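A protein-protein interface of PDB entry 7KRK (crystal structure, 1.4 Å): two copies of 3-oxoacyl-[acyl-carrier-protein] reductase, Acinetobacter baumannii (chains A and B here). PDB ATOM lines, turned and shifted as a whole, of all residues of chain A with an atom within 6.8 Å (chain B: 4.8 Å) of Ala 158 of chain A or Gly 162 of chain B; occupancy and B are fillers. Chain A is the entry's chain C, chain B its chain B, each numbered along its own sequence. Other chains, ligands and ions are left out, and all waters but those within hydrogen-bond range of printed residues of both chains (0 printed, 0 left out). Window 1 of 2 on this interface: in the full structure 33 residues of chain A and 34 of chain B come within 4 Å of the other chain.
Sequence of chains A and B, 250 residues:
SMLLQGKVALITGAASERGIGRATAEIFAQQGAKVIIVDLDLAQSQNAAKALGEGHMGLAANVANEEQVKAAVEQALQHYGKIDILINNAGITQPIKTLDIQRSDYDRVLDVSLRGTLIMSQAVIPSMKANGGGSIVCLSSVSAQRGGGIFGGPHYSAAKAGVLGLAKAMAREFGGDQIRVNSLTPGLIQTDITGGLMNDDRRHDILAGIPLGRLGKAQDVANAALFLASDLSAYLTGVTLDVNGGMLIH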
ATOM      1  N   TYR A 106     -18.109 -15.601  18.056  1.00  0.00           N
ATOM      2  CA  TYR A 106     -17.614 -14.238  18.197  1.00  0.00           C
ATOM      3  C   TYR A 106     -18.523 -13.427  19.109  1.00  0.00           C
ATOM      4  O   TYR A 106     -18.059 -12.774  20.050  1.00  0.00           O
ATOM      5  CB  TYR A 106     -17.533 -13.617  16.801  1.00  0.00           C
ATOM      6  CG  TYR A 106     -17.210 -12.140  16.725  1.00  0.00           C
ATOM      7  CD1 TYR A 106     -18.199 -11.182  16.913  1.00  0.00           C
ATOM      8  CD2 TYR A 106     -15.930 -11.705  16.408  1.00  0.00           C
ATOM      9  CE1 TYR A 106     -17.915  -9.832  16.818  1.00  0.00           C
ATOM     10  CE2 TYR A 106     -15.637 -10.355  16.306  1.00  0.00           C
ATOM     11  CZ  TYR A 106     -16.632  -9.424  16.513  1.00  0.00           C
ATOM     12  OH  TYR A 106     -16.345  -8.082  16.412  1.00  0.00           O
ATOM     13  N   LEU A 110     -17.155 -11.971  22.666  1.00  0.00           N
ATOM     14  CA  LEU A 110     -17.015 -10.520  22.724  1.00  0.00           C
ATOM     15  C   LEU A 110     -18.036  -9.886  23.662  1.00  0.00           C
ATOM     16  O   LEU A 110     -17.725  -8.891  24.326  1.00  0.00           O
ATOM     17  CB  LEU A 110     -17.131  -9.919  21.322  1.00  0.00           C
ATOM     18  CG  LEU A 110     -15.843  -9.787  20.503  1.00  0.00           C
ATOM     19  CD1 LEU A 110     -14.900  -8.772  21.139  1.00  0.00           C
ATOM     20  CD2 LEU A 110     -15.158 -11.136  20.331  1.00  0.00           C
ATOM     21  N   LEU A 114     -15.936  -7.881  26.288  1.00  0.00           N
ATOM     22  CA  LEU A 114     -15.803  -6.502  25.830  1.00  0.00           C
ATOM     23  C   LEU A 114     -17.080  -5.700  26.062  1.00  0.00           C
ATOM     24  O   LEU A 114     -17.054  -4.665  26.735  1.00  0.00           O
ATOM     25  CB  LEU A 114     -15.375  -6.452  24.361  1.00  0.00           C
ATOM     26  CG  LEU A 114     -15.134  -5.034  23.834  1.00  0.00           C
ATOM     27  CD1 LEU A 114     -14.099  -4.303  24.680  1.00  0.00           C
ATOM     28  CD2 LEU A 114     -14.703  -5.075  22.378  1.00  0.00           C
ATOM     29  N   SER A 143      -3.075 -13.722  26.417  1.00  0.00           N
ATOM     30  CA  SER A 143      -3.426 -14.074  25.045  1.00  0.00           C
ATOM     31  C   SER A 143      -3.652 -12.835  24.190  1.00  0.00           C
ATOM     32  O   SER A 143      -3.409 -12.865  22.978  1.00  0.00           O
ATOM     33  CB  SER A 143      -4.673 -14.958  25.033  1.00  0.00           C
ATOM     34  OG  SER A 143      -4.399 -16.232  25.594  1.00  0.00           O
ATOM     35  N   ALA A 144      -4.117 -11.741  24.797  1.00  0.00           N
ATOM     36  CA  ALA A 144      -4.311 -10.496  24.065  1.00  0.00           C
ATOM     37  C   ALA A 144      -2.993  -9.863  23.652  1.00  0.00           C
ATOM     38  O   ALA A 144      -2.964  -9.089  22.688  1.00  0.00           O
ATOM     39  CB  ALA A 144      -5.082  -9.503  24.934  1.00  0.00           C
ATOM     40  N   GLY A 153      -9.282 -19.103  21.942  1.00  0.00           N
ATOM     41  CA  GLY A 153      -9.072 -18.908  20.539  1.00  0.00           C
ATOM     42  C   GLY A 153      -8.865 -17.447  20.181  1.00  0.00           C
ATOM     43  O   GLY A 153      -8.894 -16.555  21.040  1.00  0.00           O
ATOM     44  N   PRO A 154      -8.648 -17.195  18.891  1.00  0.00           N
ATOM     45  CA  PRO A 154      -8.324 -15.827  18.455  1.00  0.00           C
ATOM     46  C   PRO A 154      -9.384 -14.796  18.791  1.00  0.00           C
ATOM     47  O   PRO A 154      -9.045 -13.621  18.980  1.00  0.00           O
ATOM     48  CB  PRO A 154      -8.140 -15.979  16.938  1.00  0.00           C
ATOM     49  CG  PRO A 154      -7.744 -17.405  16.755  1.00  0.00           C
ATOM     50  CD  PRO A 154      -8.484 -18.175  17.802  1.00  0.00           C
ATOM     51  N   HIS A 155     -10.660 -15.184  18.840  1.00  0.00           N
ATOM     52  CA  HIS A 155     -11.699 -14.237  19.230  1.00  0.00           C
ATOM     53  C   HIS A 155     -11.605 -13.874  20.707  1.00  0.00           C
ATOM     54  O   HIS A 155     -11.983 -12.762  21.094  1.00  0.00           O
ATOM     55  CB  HIS A 155     -13.095 -14.752  18.861  1.00  0.00           C
ATOM     56  CG  HIS A 155     -13.438 -16.097  19.427  1.00  0.00           C
ATOM     57  ND1 HIS A 155     -12.510 -17.101  19.608  1.00  0.00           N
ATOM     58  CD2 HIS A 155     -14.625 -16.610  19.831  1.00  0.00           C
ATOM     59  CE1 HIS A 155     -13.107 -18.167  20.108  1.00  0.00           C
ATOM     60  NE2 HIS A 155     -14.391 -17.896  20.251  1.00  0.00           N
ATOM     61  N   TYR A 156     -11.094 -14.782  21.542  1.00  0.00           N
ATOM     62  CA  TYR A 156     -10.819 -14.436  22.931  1.00  0.00           C
ATOM     63  C   TYR A 156      -9.630 -13.488  23.028  1.00  0.00           C
ATOM     64  O   TYR A 156      -9.674 -12.497  23.767  1.00  0.00           O
ATOM     65  CB  TYR A 156     -10.560 -15.705  23.742  1.00  0.00           C
ATOM     66  CG  TYR A 156     -10.302 -15.456  25.210  1.00  0.00           C
ATOM     67  CD1 TYR A 156     -11.353 -15.255  26.092  1.00  0.00           C
ATOM     68  CD2 TYR A 156      -9.008 -15.425  25.715  1.00  0.00           C
ATOM     69  CE1 TYR A 156     -11.126 -15.029  27.436  1.00  0.00           C
ATOM     70  CE2 TYR A 156      -8.772 -15.201  27.058  1.00  0.00           C
ATOM     71  CZ  TYR A 156      -9.835 -15.004  27.913  1.00  0.00           C
ATOM     72  OH  TYR A 156      -9.613 -14.779  29.254  1.00  0.00           O
ATOM     73  N   SER A 157      -8.557 -13.774  22.289  1.00  0.00           N
ATOM     74  CA  SER A 157      -7.433 -12.848  22.233  1.00  0.00           C
ATOM     75  C   SER A 157      -7.895 -11.472  21.776  1.00  0.00           C
ATOM     76  O   SER A 157      -7.483 -10.448  22.337  1.00  0.00           O
ATOM     77  CB  SER A 157      -6.361 -13.393  21.291  1.00  0.00           C
ATOM     78  OG  SER A 157      -5.885 -14.651  21.737  1.00  0.00           O
ATOM     79  N   ALA A 158      -8.771 -11.430  20.771  1.00  0.00           N
ATOM     80  CA  ALA A 158      -9.281 -10.156  20.277  1.00  0.00           C
ATOM     81  C   ALA A 158     -10.136  -9.462  21.327  1.00  0.00           C
ATOM     82  O   ALA A 158      -9.986  -8.258  21.569  1.00  0.00           O
ATOM     83  CB  ALA A 158     -10.090 -10.382  19.002  1.00  0.00           C
ATOM     84  N   ALA A 159     -11.049 -10.201  21.958  1.00  0.00           N
ATOM     85  CA  ALA A 159     -11.917  -9.602  22.966  1.00  0.00           C
ATOM     86  C   ALA A 159     -11.097  -9.016  24.107  1.00  0.00           C
ATOM     87  O   ALA A 159     -11.351  -7.891  24.556  1.00  0.00           O
ATOM     88  CB  ALA A 159     -12.900 -10.646  23.495  1.00  0.00           C
ATOM     89  N   LYS A 160     -10.109  -9.766  24.593  1.00  0.00           N
ATOM     90  CA  LYS A 160      -9.318  -9.293  25.723  1.00  0.00           C
ATOM     91  C   LYS A 160      -8.369  -8.172  25.321  1.00  0.00           C
ATOM     92  O   LYS A 160      -8.018  -7.335  26.160  1.00  0.00           O
ATOM     93  CB  LYS A 160      -8.566 -10.455  26.372  1.00  0.00           C
ATOM     94  CG  LYS A 160      -9.473 -11.472  27.058  1.00  0.00           C
ATOM     95  CD  LYS A 160     -10.478 -10.801  27.986  1.00  0.00           C
ATOM     96  CE  LYS A 160     -10.926 -11.735  29.096  1.00  0.00           C
ATOM     97  NZ  LYS A 160     -11.926 -11.100  29.997  1.00  0.00           N
ATOM     98  N   ALA A 161      -7.947  -8.129  24.055  1.00  0.00           N
ATOM     99  CA  ALA A 161      -7.191  -6.975  23.581  1.00  0.00           C
ATOM    100  C   ALA A 161      -8.091  -5.751  23.478  1.00  0.00           C
ATOM    101  O   ALA A 161      -7.682  -4.640  23.833  1.00  0.00           O
ATOM    102  CB  ALA A 161      -6.543  -7.281  22.230  1.00  0.00           C
ATOM    103  N   GLY A 162      -9.324  -5.940  23.003  1.00  0.00           N
ATOM    104  CA  GLY A 162     -10.284  -4.852  23.001  1.00  0.00           C
ATOM    105  C   GLY A 162     -10.510  -4.278  24.386  1.00  0.00           C
ATOM    106  O   GLY A 162     -10.654  -3.065  24.549  1.00  0.00           O
ATOM    107  N   VAL A 163     -10.541  -5.143  25.403  1.00  0.00           N
ATOM    108  CA  VAL A 163     -10.674  -4.677  26.782  1.00  0.00           C
ATOM    109  C   VAL A 163      -9.536  -3.731  27.141  1.00  0.00           C
ATOM    110  O   VAL A 163      -9.744  -2.711  27.808  1.00  0.00           O
ATOM    111  CB  VAL A 163     -10.759  -5.876  27.746  1.00  0.00           C
ATOM    112  CG1 VAL A 163     -10.558  -5.432  29.192  1.00  0.00           C
ATOM    113  CG2 VAL A 163     -12.093  -6.587  27.585  1.00  0.00           C
ATOM    114  N   GLY A 165      -7.790  -1.780  25.088  1.00  0.00           N
ATOM    115  CA  GLY A 165      -8.028  -0.508  24.430  1.00  0.00           C
ATOM    116  C   GLY A 165      -9.127   0.290  25.104  1.00  0.00           C
ATOM    117  O   GLY A 165      -9.002   1.504  25.295  1.00  0.00           O
ATOM    118  N   LEU B 114     -13.204  -4.887  13.593  1.00  0.00           N
ATOM    119  CA  LEU B 114     -12.844  -6.178  14.168  1.00  0.00           C
ATOM    120  C   LEU B 114     -13.530  -7.330  13.443  1.00  0.00           C
ATOM    121  O   LEU B 114     -12.863  -8.232  12.929  1.00  0.00           O
ATOM    122  CB  LEU B 114     -13.140  -6.213  15.670  1.00  0.00           C
ATOM    123  CG  LEU B 114     -12.748  -7.533  16.343  1.00  0.00           C
ATOM    124  CD1 LEU B 114     -11.265  -7.834  16.143  1.00  0.00           C
ATOM    125  CD2 LEU B 114     -13.092  -7.508  17.819  1.00  0.00           C
ATOM    126  N   ALA B 158     -11.223   0.462  21.453  1.00  0.00           N
ATOM    127  CA  ALA B 158     -11.410  -0.955  21.749  1.00  0.00           C
ATOM    128  C   ALA B 158     -11.387  -1.790  20.477  1.00  0.00           C
ATOM    129  O   ALA B 158     -10.730  -2.835  20.421  1.00  0.00           O
ATOM    130  CB  ALA B 158     -12.728  -1.157  22.495  1.00  0.00           C
ATOM    131  N   ALA B 159     -12.110  -1.351  19.444  1.00  0.00           N
ATOM    132  CA  ALA B 159     -12.147  -2.107  18.197  1.00  0.00           C
ATOM    133  C   ALA B 159     -10.751  -2.242  17.605  1.00  0.00           C
ATOM    134  O   ALA B 159     -10.351  -3.327  17.165  1.00  0.00           O
ATOM    135  CB  ALA B 159     -13.084  -1.427  17.201  1.00  0.00           C
ATOM    136  N   LYS B 160      -9.996  -1.143  17.580  1.00  0.00           N
ATOM    137  CA  LYS B 160      -8.668  -1.180  16.980  1.00  0.00           C
ATOM    138  C   LYS B 160      -7.676  -1.942  17.849  1.00  0.00           C
ATOM    139  O   LYS B 160      -6.720  -2.525  17.326  1.00  0.00           O
ATOM    140  CB  LYS B 160      -8.181   0.239  16.685  1.00  0.00           C
ATOM    141  CG  LYS B 160      -8.977   0.959  15.598  1.00  0.00           C
ATOM    142  CD  LYS B 160      -9.122   0.104  14.346  1.00  0.00           C
ATOM    143  CE  LYS B 160      -9.377   0.944  13.108  1.00  0.00           C
ATOM    144  NZ  LYS B 160      -9.474   0.100  11.885  1.00  0.00           N
ATOM    145  N   ALA B 161      -7.884  -1.964  19.168  1.00  0.00           N
ATOM    146  CA  ALA B 161      -7.076  -2.831  20.020  1.00  0.00           C
ATOM    147  C   ALA B 161      -7.446  -4.294  19.808  1.00  0.00           C
ATOM    148  O   ALA B 161      -6.569  -5.166  19.784  1.00  0.00           O
ATOM    149  CB  ALA B 161      -7.248  -2.440  21.486  1.00  0.00           C
ATOM    150  N   GLY B 162      -8.738  -4.579  19.647  1.00  0.00           N
ATOM    151  CA  GLY B 162      -9.148  -5.933  19.324  1.00  0.00           C
ATOM    152  C   GLY B 162      -8.524  -6.428  18.034  1.00  0.00           C
ATOM    153  O   GLY B 162      -8.156  -7.600  17.920  1.00  0.00           O
ATOM    154  N   VAL B 163      -8.392  -5.539  17.046  1.00  0.00           N
ATOM    155  CA  VAL B 163      -7.729  -5.903  15.797  1.00  0.00           C
ATOM    156  C   VAL B 163      -6.305  -6.372  16.067  1.00  0.00           C
ATOM    157  O   VAL B 163      -5.841  -7.356  15.480  1.00  0.00           O
ATOM    158  CB  VAL B 163      -7.770  -4.725  14.806  1.00  0.00           C
ATOM    159  CG1 VAL B 163      -6.773  -4.942  13.670  1.00  0.00           C
ATOM    160  CG2 VAL B 163      -9.176  -4.540  14.260  1.00  0.00           C
ATOM    161  N   LEU B 164      -5.590  -5.678  16.956  1.00  0.00           N
ATOM    162  CA  LEU B 164      -4.228  -6.089  17.291  1.00  0.00           C
ATOM    163  C   LEU B 164      -4.213  -7.485  17.897  1.00  0.00           C
ATOM    164  O   LEU B 164      -3.394  -8.332  17.520  1.00  0.00           O
ATOM    165  CB  LEU B 164      -3.600  -5.088  18.261  1.00  0.00           C
ATOM    166  CG  LEU B 164      -3.378  -3.674  17.728  1.00  0.00           C
ATOM    167  CD1 LEU B 164      -2.831  -2.773  18.824  1.00  0.00           C
ATOM    168  CD2 LEU B 164      -2.436  -3.688  16.534  1.00  0.00           C
ATOM    169  N   GLY B 165      -5.107  -7.743  18.852  1.00  0.00           N
ATOM    170  CA  GLY B 165      -5.157  -9.061  19.460  1.00  0.00           C
ATOM    171  C   GLY B 165      -5.457 -10.150  18.450  1.00  0.00           C
ATOM    172  O   GLY B 165      -4.841 -11.219  18.471  1.00  0.00           O
ATOM    173  N   LEU B 166      -6.408  -9.893  17.549  1.00  0.00           N
ATOM    174  CA  LEU B 166      -6.737 -10.872  16.518  1.00  0.00           C
ATOM    175  C   LEU B 166      -5.565 -11.077  15.569  1.00  0.00           C
ATOM    176  O   LEU B 166      -5.227 -12.216  15.223  1.00  0.00           O
ATOM    177  CB  LEU B 166      -7.972 -10.410  15.745  1.00  0.00           C
ATOM    178  CG  LEU B 166      -8.436 -11.326  14.610  1.00  0.00           C
ATOM    179  CD1 LEU B 166      -8.902 -12.666  15.159  1.00  0.00           C
ATOM    180  CD2 LEU B 166      -9.538 -10.654  13.804  1.00  0.00           C
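Tyr 106 of chain A touches Leu 114 of chain B. CD2 of Leu 114 of chain B touches CD1 of Leu 110 of chain A (3.99 Å). Ala 144 of chain A touches Gly 165 of chain B (O to CA, 3.9 Å). Pro 154 of chain A touches Leu 166 of chain B. Gly 165 of chain B touches Ser 157 of chain A (O to CB, 3.9 Å). Ala 158 of chain A touches Gly 162 of chain B (O to CA, 3.3 Å). Ala 158 of chain A touches Leu 166 of chain B. Ala 161 of chain A touches Gly 165 of chain B. Ala 158 of chain B touches Gly 162 of chain A. Ala 161 of chain B touches Gly 165 of chain A (CB to CA, 3.6 Å).
OG of Ser 157 of chain A sits at hydrogen-bond distance from O of Ser 143 of chain A (3.3 Å).
Of the printed residues of chain B, Ala 158 of chain A touches Gly 162 and Leu 166. Of the printed residues of chain B, Ala 161 of chain A touches Ala 161 and Gly 165. Of the printed residues of chain A, Ala 158 of chain B touches Gly 162 (3.3 Å). Printed residues of chain A within 4 Å of Gly 162 of chain B: Ala 158 (3.3 Å) and Gly 162 (3.7 Å). The nearest printed residue of chain B that does not touch Ala 158 of chain A is Leu 114 of chain B (4.01 Å). The nearest residue of chain A that does not touch Gly 162 of chain B is Ala 161 of chain A (4.1 Å).
Ala 158 of chain A touches Gly 162 of chain B, and with the chains exchanged Gly 162 of chain A touches Ala 158 of chain B. Ala 161 of chain A touches its own counterpart, Ala 161 of chain B. Ala 161 of chain A touches Gly 165 of chain B, and with the chains exchanged Gly 165 of chain A touches Ala 161 of chain B. Gly 162 of chain A touches its own counterpart, Gly 162 of chain B. Positions printed for both chains: 114, 158, 159, 160, 161, 162, 163 and 165. Of the 12 pairs that touch across the chains among the printed residues, 6 have their exchanged pair printed and touching as well.
Printed residues of chain A that touch a printed residue of chain B: Tyr 106, Leu 110, Ala 144, Pro 154, Ser 157, Ala 158, Ala 161, Gly 162 and Gly 165. Hydrophobic or aromatic side chains of chain A that line the printed part of chain B: Tyr 106, Leu 110, Pro 154, Ala 158 and Ala 161. Of the 10 printed residues of chain B, 6 touch a printed residue of chain A. Among the printed residues, no Asp or Glu carboxylate lies within 4 Å of a Lys or Arg side-chain nitrogen of the other chain.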
